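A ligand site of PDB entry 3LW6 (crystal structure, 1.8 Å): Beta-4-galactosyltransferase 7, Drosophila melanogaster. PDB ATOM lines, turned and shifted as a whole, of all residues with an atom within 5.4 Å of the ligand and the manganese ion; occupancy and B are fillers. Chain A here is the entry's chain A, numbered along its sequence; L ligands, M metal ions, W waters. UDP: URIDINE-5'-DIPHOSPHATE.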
ATOM      1  N   VAL A  57       9.870  -2.587   7.257  1.00  0.00           N
ATOM      2  CA  VAL A  57      11.141  -2.672   7.968  1.00  0.00           C
ATOM      3  C   VAL A  57      12.179  -1.848   7.206  1.00  0.00           C
ATOM      4  O   VAL A  57      12.704  -2.278   6.172  1.00  0.00           O
ATOM      5  CB  VAL A  57      11.633  -4.130   8.073  1.00  0.00           C
ATOM      6  CG1 VAL A  57      12.892  -4.185   8.924  1.00  0.00           C
ATOM      7  CG2 VAL A  57      10.548  -5.024   8.746  1.00  0.00           C
ATOM      8  N   PRO A  58      12.482  -0.663   7.687  1.00  0.00           N
ATOM      9  CA  PRO A  58      13.549   0.186   7.108  1.00  0.00           C
ATOM     10  C   PRO A  58      14.859  -0.578   7.190  1.00  0.00           C
ATOM     11  O   PRO A  58      15.106  -1.272   8.201  1.00  0.00           O
ATOM     12  CB  PRO A  58      13.528   1.451   7.959  1.00  0.00           C
ATOM     13  CG  PRO A  58      12.684   1.104   9.127  1.00  0.00           C
ATOM     14  CD  PRO A  58      11.915  -0.121   8.942  1.00  0.00           C
ATOM     15  N   PHE A  59      15.641  -0.557   6.098  1.00  0.00           N
ATOM     16  CA  PHE A  59      16.754  -1.514   5.997  1.00  0.00           C
ATOM     17  C   PHE A  59      17.883  -0.984   5.151  1.00  0.00           C
ATOM     18  O   PHE A  59      17.668  -0.566   4.002  1.00  0.00           O
ATOM     19  CB  PHE A  59      16.262  -2.845   5.392  1.00  0.00           C
ATOM     20  CG  PHE A  59      17.357  -3.931   5.349  1.00  0.00           C
ATOM     21  CD1 PHE A  59      17.416  -4.900   6.345  1.00  0.00           C
ATOM     22  CD2 PHE A  59      18.255  -3.977   4.286  1.00  0.00           C
ATOM     23  CE1 PHE A  59      18.383  -5.911   6.255  1.00  0.00           C
ATOM     24  CE2 PHE A  59      19.299  -4.951   4.228  1.00  0.00           C
ATOM     25  CZ  PHE A  59      19.333  -5.905   5.221  1.00  0.00           C
ATOM     26  N   ARG A  60      19.105  -1.080   5.713  1.00  0.00           N
ATOM     27  CA  ARG A  60      20.306  -0.976   4.901  1.00  0.00           C
ATOM     28  C   ARG A  60      21.425  -1.598   5.742  1.00  0.00           C
ATOM     29  O   ARG A  60      21.643  -1.181   6.934  1.00  0.00           O
ATOM     30  CB  ARG A  60      20.670   0.462   4.666  1.00  0.00           C
ATOM     31  CG  ARG A  60      22.009   0.577   3.912  1.00  0.00           C
ATOM     32  CD  ARG A  60      22.471   2.013   4.078  1.00  0.00           C
ATOM     33  NE  ARG A  60      21.955   2.709   2.928  1.00  0.00           N
ATOM     34  CZ  ARG A  60      21.976   4.014   2.740  1.00  0.00           C
ATOM     35  NH1 ARG A  60      22.427   4.884   3.669  1.00  0.00           N
ATOM     36  NH2 ARG A  60      21.520   4.448   1.564  1.00  0.00           N
ATOM     37  N   ASP A  61      22.112  -2.547   5.115  1.00  0.00           N
ATOM     38  CA  ASP A  61      23.237  -3.271   5.786  1.00  0.00           C
ATOM     39  C   ASP A  61      22.858  -3.888   7.176  1.00  0.00           C
ATOM     40  O   ASP A  61      23.577  -3.657   8.154  1.00  0.00           O
ATOM     41  CB  ASP A  61      24.362  -2.211   6.079  1.00  0.00           C
ATOM     42  CG  ASP A  61      24.986  -1.628   4.772  1.00  0.00           C
ATOM     43  OD1 ASP A  61      24.770  -2.215   3.692  1.00  0.00           O
ATOM     44  OD2 ASP A  61      25.627  -0.559   4.842  1.00  0.00           O
ATOM     45  N   ARG A  62      21.780  -4.653   7.255  1.00  0.00           N
ATOM     46  CA  ARG A  62      21.337  -5.235   8.535  1.00  0.00           C
ATOM     47  C   ARG A  62      20.960  -6.680   8.281  1.00  0.00           C
ATOM     48  O   ARG A  62      20.040  -7.230   8.898  1.00  0.00           O
ATOM     49  CB  ARG A  62      20.146  -4.448   9.147  1.00  0.00           C
ATOM     50  CG  ARG A  62      20.515  -3.029   9.526  1.00  0.00           C
ATOM     51  CD  ARG A  62      21.480  -2.924  10.752  1.00  0.00           C
ATOM     52  NE  ARG A  62      21.706  -1.531  11.208  1.00  0.00           N
ATOM     53  CZ  ARG A  62      22.601  -0.713  10.664  1.00  0.00           C
ATOM     54  NH1 ARG A  62      23.404  -1.119   9.644  1.00  0.00           N
ATOM     55  NH2 ARG A  62      22.726   0.521  11.123  1.00  0.00           N
ATOM     56  N   PHE A  97      20.886   7.419   5.501  1.00  0.00           N
ATOM     57  CA  PHE A  97      19.734   6.581   5.720  1.00  0.00           C
ATOM     58  C   PHE A  97      18.500   7.451   6.069  1.00  0.00           C
ATOM     59  O   PHE A  97      18.564   8.295   6.980  1.00  0.00           O
ATOM     60  CB  PHE A  97      20.033   5.596   6.860  1.00  0.00           C
ATOM     61  CG  PHE A  97      19.006   4.489   6.959  1.00  0.00           C
ATOM     62  CD1 PHE A  97      18.931   3.507   5.997  1.00  0.00           C
ATOM     63  CD2 PHE A  97      18.070   4.518   7.976  1.00  0.00           C
ATOM     64  CE1 PHE A  97      17.959   2.455   6.064  1.00  0.00           C
ATOM     65  CE2 PHE A  97      17.104   3.502   8.062  1.00  0.00           C
ATOM     66  CZ  PHE A  97      17.035   2.476   7.098  1.00  0.00           C
ATOM     67  N   ARG A  99      14.942   6.700   7.230  1.00  0.00           N
ATOM     68  CA  ARG A  99      13.926   5.805   7.718  1.00  0.00           C
ATOM     69  C   ARG A  99      12.509   6.226   7.315  1.00  0.00           C
ATOM     70  O   ARG A  99      11.700   5.375   6.853  1.00  0.00           O
ATOM     71  CB  ARG A  99      13.997   5.785   9.283  1.00  0.00           C
ATOM     72  CG  ARG A  99      12.984   4.807   9.932  1.00  0.00           C
ATOM     73  CD  ARG A  99      13.284   4.735  11.468  1.00  0.00           C
ATOM     74  NE  ARG A  99      12.333   3.829  12.148  1.00  0.00           N
ATOM     75  CZ  ARG A  99      11.218   4.246  12.771  1.00  0.00           C
ATOM     76  NH1 ARG A  99      10.902   5.543  12.814  1.00  0.00           N
ATOM     77  NH2 ARG A  99      10.446   3.329  13.382  1.00  0.00           N
ATOM     78  N   HIS A 120       8.623  -0.783  11.663  1.00  0.00           N
ATOM     79  CA  HIS A 120       9.227  -1.685  12.625  1.00  0.00           C
ATOM     80  C   HIS A 120      10.776  -1.734  12.445  1.00  0.00           C
ATOM     81  O   HIS A 120      11.251  -2.195  11.421  1.00  0.00           O
ATOM     82  CB  HIS A 120       8.680  -3.113  12.430  1.00  0.00           C
ATOM     83  CG  HIS A 120       8.793  -3.958  13.677  1.00  0.00           C
ATOM     84  ND1 HIS A 120       7.729  -4.591  14.277  1.00  0.00           N
ATOM     85  CD2 HIS A 120       9.884  -4.236  14.446  1.00  0.00           C
ATOM     86  CE1 HIS A 120       8.147  -5.204  15.393  1.00  0.00           C
ATOM     87  NE2 HIS A 120       9.465  -5.027  15.489  1.00  0.00           N
ATOM     88  N   ASP A 121      11.518  -1.302  13.442  1.00  0.00           N
ATOM     89  CA  ASP A 121      12.977  -1.470  13.379  1.00  0.00           C
ATOM     90  C   ASP A 121      13.352  -2.918  13.287  1.00  0.00           C
ATOM     91  O   ASP A 121      12.765  -3.763  13.945  1.00  0.00           O
ATOM     92  CB  ASP A 121      13.647  -0.784  14.557  1.00  0.00           C
ATOM     93  CG  ASP A 121      13.460   0.768  14.505  1.00  0.00           C
ATOM     94  OD1 ASP A 121      12.864   1.287  13.538  1.00  0.00           O
ATOM     95  OD2 ASP A 121      13.890   1.416  15.459  1.00  0.00           O
ATOM     96  N   VAL A 122      14.429  -3.203  12.548  1.00  0.00           N
ATOM     97  CA  VAL A 122      14.769  -4.627  12.289  1.00  0.00           C
ATOM     98  C   VAL A 122      15.468  -5.261  13.519  1.00  0.00           C
ATOM     99  O   VAL A 122      15.625  -6.473  13.560  1.00  0.00           O
ATOM    100  CB  VAL A 122      15.699  -4.712  11.067  1.00  0.00           C
ATOM    101  CG1 VAL A 122      17.070  -4.101  11.431  1.00  0.00           C
ATOM    102  CG2 VAL A 122      15.791  -6.108  10.515  1.00  0.00           C
ATOM    103  N   ASP A 123      15.889  -4.429  14.482  1.00  0.00           N
ATOM    104  CA  ASP A 123      16.771  -4.906  15.569  1.00  0.00           C
ATOM    105  C   ASP A 123      16.025  -4.938  16.913  1.00  0.00           C
ATOM    106  O   ASP A 123      16.628  -5.099  17.958  1.00  0.00           O
ATOM    107  CB  ASP A 123      18.060  -4.025  15.708  1.00  0.00           C
ATOM    108  CG  ASP A 123      17.742  -2.590  16.059  1.00  0.00           C
ATOM    109  OD1 ASP A 123      16.517  -2.313  16.217  1.00  0.00           O
ATOM    110  OD2 ASP A 123      18.620  -1.678  16.143  1.00  0.00           O
ATOM    111  N   HIS A 150      10.694   0.462  26.206  1.00  0.00           N
ATOM    112  CA  HIS A 150      11.896   0.535  25.395  1.00  0.00           C
ATOM    113  C   HIS A 150      13.198   0.551  26.225  1.00  0.00           C
ATOM    114  O   HIS A 150      13.317   1.270  27.220  1.00  0.00           O
ATOM    115  CB  HIS A 150      11.829   1.786  24.498  1.00  0.00           C
ATOM    116  CG  HIS A 150      12.856   1.770  23.401  1.00  0.00           C
ATOM    117  ND1 HIS A 150      12.550   1.483  22.088  1.00  0.00           N
ATOM    118  CD2 HIS A 150      14.197   1.949  23.445  1.00  0.00           C
ATOM    119  CE1 HIS A 150      13.658   1.524  21.362  1.00  0.00           C
ATOM    120  NE2 HIS A 150      14.674   1.817  22.161  1.00  0.00           N
ATOM    121  N   LYS A 152      16.039   1.896  25.722  1.00  0.00           N
ATOM    122  CA  LYS A 152      16.936   3.045  25.609  1.00  0.00           C
ATOM    123  C   LYS A 152      16.237   4.375  25.699  1.00  0.00           C
ATOM    124  O   LYS A 152      16.762   5.336  26.286  1.00  0.00           O
ATOM    125  CB  LYS A 152      17.694   2.907  24.267  1.00  0.00           C
ATOM    126  CG  LYS A 152      18.864   3.778  24.141  1.00  0.00           C
ATOM    127  CD  LYS A 152      19.582   3.543  22.805  1.00  0.00           C
ATOM    128  CE  LYS A 152      20.611   4.623  22.648  1.00  0.00           C
ATOM    129  NZ  LYS A 152      21.765   4.274  23.546  1.00  0.00           N
ATOM    130  N   TYR A 153      15.071   4.493  25.063  1.00  0.00           N
ATOM    131  CA  TYR A 153      14.398   5.782  24.987  1.00  0.00           C
ATOM    132  C   TYR A 153      13.173   5.873  25.879  1.00  0.00           C
ATOM    133  O   TYR A 153      12.272   5.070  25.751  1.00  0.00           O
ATOM    134  CB  TYR A 153      14.014   6.110  23.516  1.00  0.00           C
ATOM    135  CG  TYR A 153      15.222   6.049  22.609  1.00  0.00           C
ATOM    136  CD1 TYR A 153      16.325   6.865  22.845  1.00  0.00           C
ATOM    137  CD2 TYR A 153      15.271   5.174  21.512  1.00  0.00           C
ATOM    138  CE1 TYR A 153      17.452   6.805  22.036  1.00  0.00           C
ATOM    139  CE2 TYR A 153      16.407   5.080  20.698  1.00  0.00           C
ATOM    140  CZ  TYR A 153      17.479   5.968  20.944  1.00  0.00           C
ATOM    141  OH  TYR A 153      18.620   5.868  20.153  1.00  0.00           O
ATOM    142  N   TRP A 183      20.283   9.799  11.351  1.00  0.00           N
ATOM    143  CA  TRP A 183      19.550   9.472  12.592  1.00  0.00           C
ATOM    144  C   TRP A 183      18.871  10.695  13.187  1.00  0.00           C
ATOM    145  O   TRP A 183      19.415  11.846  13.179  1.00  0.00           O
ATOM    146  CB  TRP A 183      20.533   8.873  13.613  1.00  0.00           C
ATOM    147  CG  TRP A 183      19.891   8.382  14.859  1.00  0.00           C
ATOM    148  CD1 TRP A 183      19.520   7.104  15.132  1.00  0.00           C
ATOM    149  CD2 TRP A 183      19.552   9.163  15.990  1.00  0.00           C
ATOM    150  NE1 TRP A 183      18.983   7.024  16.409  1.00  0.00           N
ATOM    151  CE2 TRP A 183      18.960   8.286  16.944  1.00  0.00           C
ATOM    152  CE3 TRP A 183      19.681  10.524  16.304  1.00  0.00           C
ATOM    153  CZ2 TRP A 183      18.485   8.737  18.199  1.00  0.00           C
ATOM    154  CZ3 TRP A 183      19.238  10.989  17.554  1.00  0.00           C
ATOM    155  CH2 TRP A 183      18.633  10.079  18.496  1.00  0.00           C
ATOM    156  N   HIS A 217      17.031  -5.562  22.135  1.00  0.00           N
ATOM    157  CA  HIS A 217      17.495  -4.561  21.159  1.00  0.00           C
ATOM    158  C   HIS A 217      18.904  -4.907  20.918  1.00  0.00           C
ATOM    159  O   HIS A 217      19.771  -4.415  21.609  1.00  0.00           O
ATOM    160  CB  HIS A 217      17.362  -3.150  21.738  1.00  0.00           C
ATOM    161  CG  HIS A 217      17.755  -2.025  20.780  1.00  0.00           C
ATOM    162  ND1 HIS A 217      18.254  -0.829  21.246  1.00  0.00           N
ATOM    163  CD2 HIS A 217      17.723  -1.922  19.426  1.00  0.00           C
ATOM    164  CE1 HIS A 217      18.477  -0.009  20.215  1.00  0.00           C
ATOM    165  NE2 HIS A 217      18.180  -0.651  19.109  1.00  0.00           N
ATOM    166  N   HIS A 219      21.809  -4.182  19.409  1.00  0.00           N
ATOM    167  CA  HIS A 219      22.323  -3.087  18.574  1.00  0.00           C
ATOM    168  C   HIS A 219      23.448  -2.511  19.366  1.00  0.00           C
ATOM    169  O   HIS A 219      23.236  -1.758  20.369  1.00  0.00           O
ATOM    170  CB  HIS A 219      21.223  -2.018  18.366  1.00  0.00           C
ATOM    171  CG  HIS A 219      21.668  -0.781  17.618  1.00  0.00           C
ATOM    172  ND1 HIS A 219      20.757   0.149  17.113  1.00  0.00           N
ATOM    173  CD2 HIS A 219      22.905  -0.315  17.256  1.00  0.00           C
ATOM    174  CE1 HIS A 219      21.411   1.131  16.502  1.00  0.00           C
ATOM    175  NE2 HIS A 219      22.716   0.882  16.576  1.00  0.00           N
ATOM    176  N   ARG A 226      25.268   5.072  14.680  1.00  0.00           N
ATOM    177  CA  ARG A 226      24.135   5.952  14.378  1.00  0.00           C
ATOM    178  C   ARG A 226      24.696   7.162  13.686  1.00  0.00           C
ATOM    179  O   ARG A 226      25.667   7.799  14.173  1.00  0.00           O
ATOM    180  CB  ARG A 226      23.420   6.394  15.664  1.00  0.00           C
ATOM    181  CG  ARG A 226      22.695   5.227  16.320  1.00  0.00           C
ATOM    182  CD  ARG A 226      21.976   5.681  17.611  1.00  0.00           C
ATOM    183  NE  ARG A 226      21.245   4.518  18.200  1.00  0.00           N
ATOM    184  CZ  ARG A 226      21.755   3.589  19.003  1.00  0.00           C
ATOM    185  NH1 ARG A 226      23.057   3.593  19.374  1.00  0.00           N
ATOM    186  NH2 ARG A 226      20.951   2.589  19.410  1.00  0.00           N
HETATM  187  N1  UDP L   1      18.471   1.178   9.896  1.00  0.00           N
HETATM  188  C2  UDP L   1      19.123   0.396   8.976  1.00  0.00           C
HETATM  189  N3  UDP L   1      20.377   0.785   8.502  1.00  0.00           N
HETATM  190  C4  UDP L   1      20.935   1.953   8.981  1.00  0.00           C
HETATM  191  C5  UDP L   1      20.260   2.770   9.936  1.00  0.00           C
HETATM  192  C6  UDP L   1      19.032   2.297  10.505  1.00  0.00           C
HETATM  193  O2  UDP L   1      18.646  -0.643   8.518  1.00  0.00           O
HETATM  194  O4  UDP L   1      22.068   2.269   8.465  1.00  0.00           O
HETATM  195  C1' UDP L   1      17.048   0.760  10.302  1.00  0.00           C
HETATM  196  C2' UDP L   1      17.005  -0.511  11.127  1.00  0.00           C
HETATM  197  O2' UDP L   1      15.747  -1.160  10.894  1.00  0.00           O
HETATM  198  C3' UDP L   1      17.152   0.092  12.520  1.00  0.00           C
HETATM  199  C4' UDP L   1      16.199   1.302  12.349  1.00  0.00           C
HETATM  200  O4' UDP L   1      16.519   1.837  11.042  1.00  0.00           O
HETATM  201  O3' UDP L   1      16.761  -0.864  13.519  1.00  0.00           O
HETATM  202  C5' UDP L   1      16.323   2.404  13.394  1.00  0.00           C
HETATM  203  O5' UDP L   1      17.707   2.808  13.404  1.00  0.00           O
HETATM  204  PA  UDP L   1      18.608   2.625  14.762  1.00  0.00           P
HETATM  205  O1A UDP L   1      18.666   1.218  15.093  1.00  0.00           O
HETATM  206  O2A UDP L   1      19.969   3.228  14.520  1.00  0.00           O
HETATM  207  O3A UDP L   1      17.790   3.495  15.846  1.00  0.00           O
HETATM  208  PB  UDP L   1      17.808   3.427  17.470  1.00  0.00           P
HETATM  209  O1B UDP L   1      18.458   2.075  17.835  1.00  0.00           O
HETATM  210  O2B UDP L   1      18.450   4.654  17.916  1.00  0.00           O
HETATM  211  O3B UDP L   1      16.369   3.377  17.747  1.00  0.00           O
HETATM  212 MN    MN M   1      18.515   0.232  17.054  1.00  0.00          MN
HETATM  213  O   HOH W   1      23.109   4.937   9.054  1.00  0.00           O
HETATM  214  O   HOH W   2      17.359   5.483  11.327  1.00  0.00           O
HETATM  215  O   HOH W   3      22.411   2.699  13.419  1.00  0.00           O
HETATM  216  O   HOH W   4      20.846  -0.022  13.344  1.00  0.00           O
HETATM  217  O   HOH W   5      14.818   1.524  18.864  1.00  0.00           O
HETATM  218  O   HOH W   6      19.820   5.104  12.406  1.00  0.00           O
HETATM  219  O   HOH W   7      16.221   0.199  16.772  1.00  0.00           O
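The guanidinium group (NH2) of Arg 62 lies close to an oxygen (O4) of the ligand.
NE1 of Trp 183 sits at hydrogen-bond distance from O2B of the ligand, at 2.9 Å.
The backbone NH (N) of Arg 60 sits at hydrogen-bond distance from an oxygen (O2) of the ligand (2.9 Å).
O2' of the ligand sits at hydrogen-bond distance from N of Val 122, 2.9 Å away.
The guanidinium group of Arg 226 lies within salt-bridge range of an oxygen (O2B) of the ligand.
OH of Tyr 153 lies within hydrogen-bond range of O2B of the ligand, 2.6 Å away.
A nitrogen (N3) of the ligand lies within hydrogen-bond range of the backbone carbonyl oxygen (O) of Arg 60.
An oxygen (O2') of the ligand lies within hydrogen-bond range of the backbone carbonyl oxygen of Pro 58 (2.8 Å).
ND1 of His 219 sits close to NH2 of Arg 226.
The backbone carbonyl oxygen of Arg 60 lies within hydrogen-bond range of the guanidinium group of Arg 62, at 3.2 Å.
The side-chain carboxylate of Asp 121 lies within salt-bridge range of the guanidinium group of Arg 99, 2.9 Å away.
CA of Phe 59 touches O2 of the ligand, 3.3 Å away.
CE2 of Phe 97 touches N1 of the ligand, at 3.3 Å.
Asp 121 touches the ligand (CB to O3', 3.3 Å).
Hydrophobic or aromatic side chains within 4 Å of the ligand: Phe 97, Val 122, Tyr 153, Trp 183, His 217 and His 219.
The nearest printed residue that does not touch the manganese ion is Arg 226 (4.1 Å).
An oxygen (O1B) of the ligand is bound to the manganese ion, at 2.0 Å.
The manganese ion is bound by the side-chain carboxylate (OD2) of Asp 123.
An oxygen (O1A) of the ligand binds the manganese ion (2.2 Å).
ND1 of His 219 binds the manganese ion, 2.2 Å away.
The manganese ion is bound by a ring nitrogen (NE2) of His 217 (2.3 Å).
Water W7 binds the manganese ion.
The manganese ion has six donor atoms within binding distance.
Water W7 lies within hydrogen-bond range of OD1 of Asp 123 (2.6 Å), OD2 of Asp 121 (2.9 Å) and O3B of the ligand (3.3 Å).
Water W5 lies within hydrogen-bond range of O3B of the ligand (2.7 Å) and NE2 of His 150 (3.3 Å).
Water W3 lies within hydrogen-bond range of an oxygen (O2A) of the ligand (2.7 Å) and the guanidinium group (NH2) of Arg 62 (3.2 Å).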
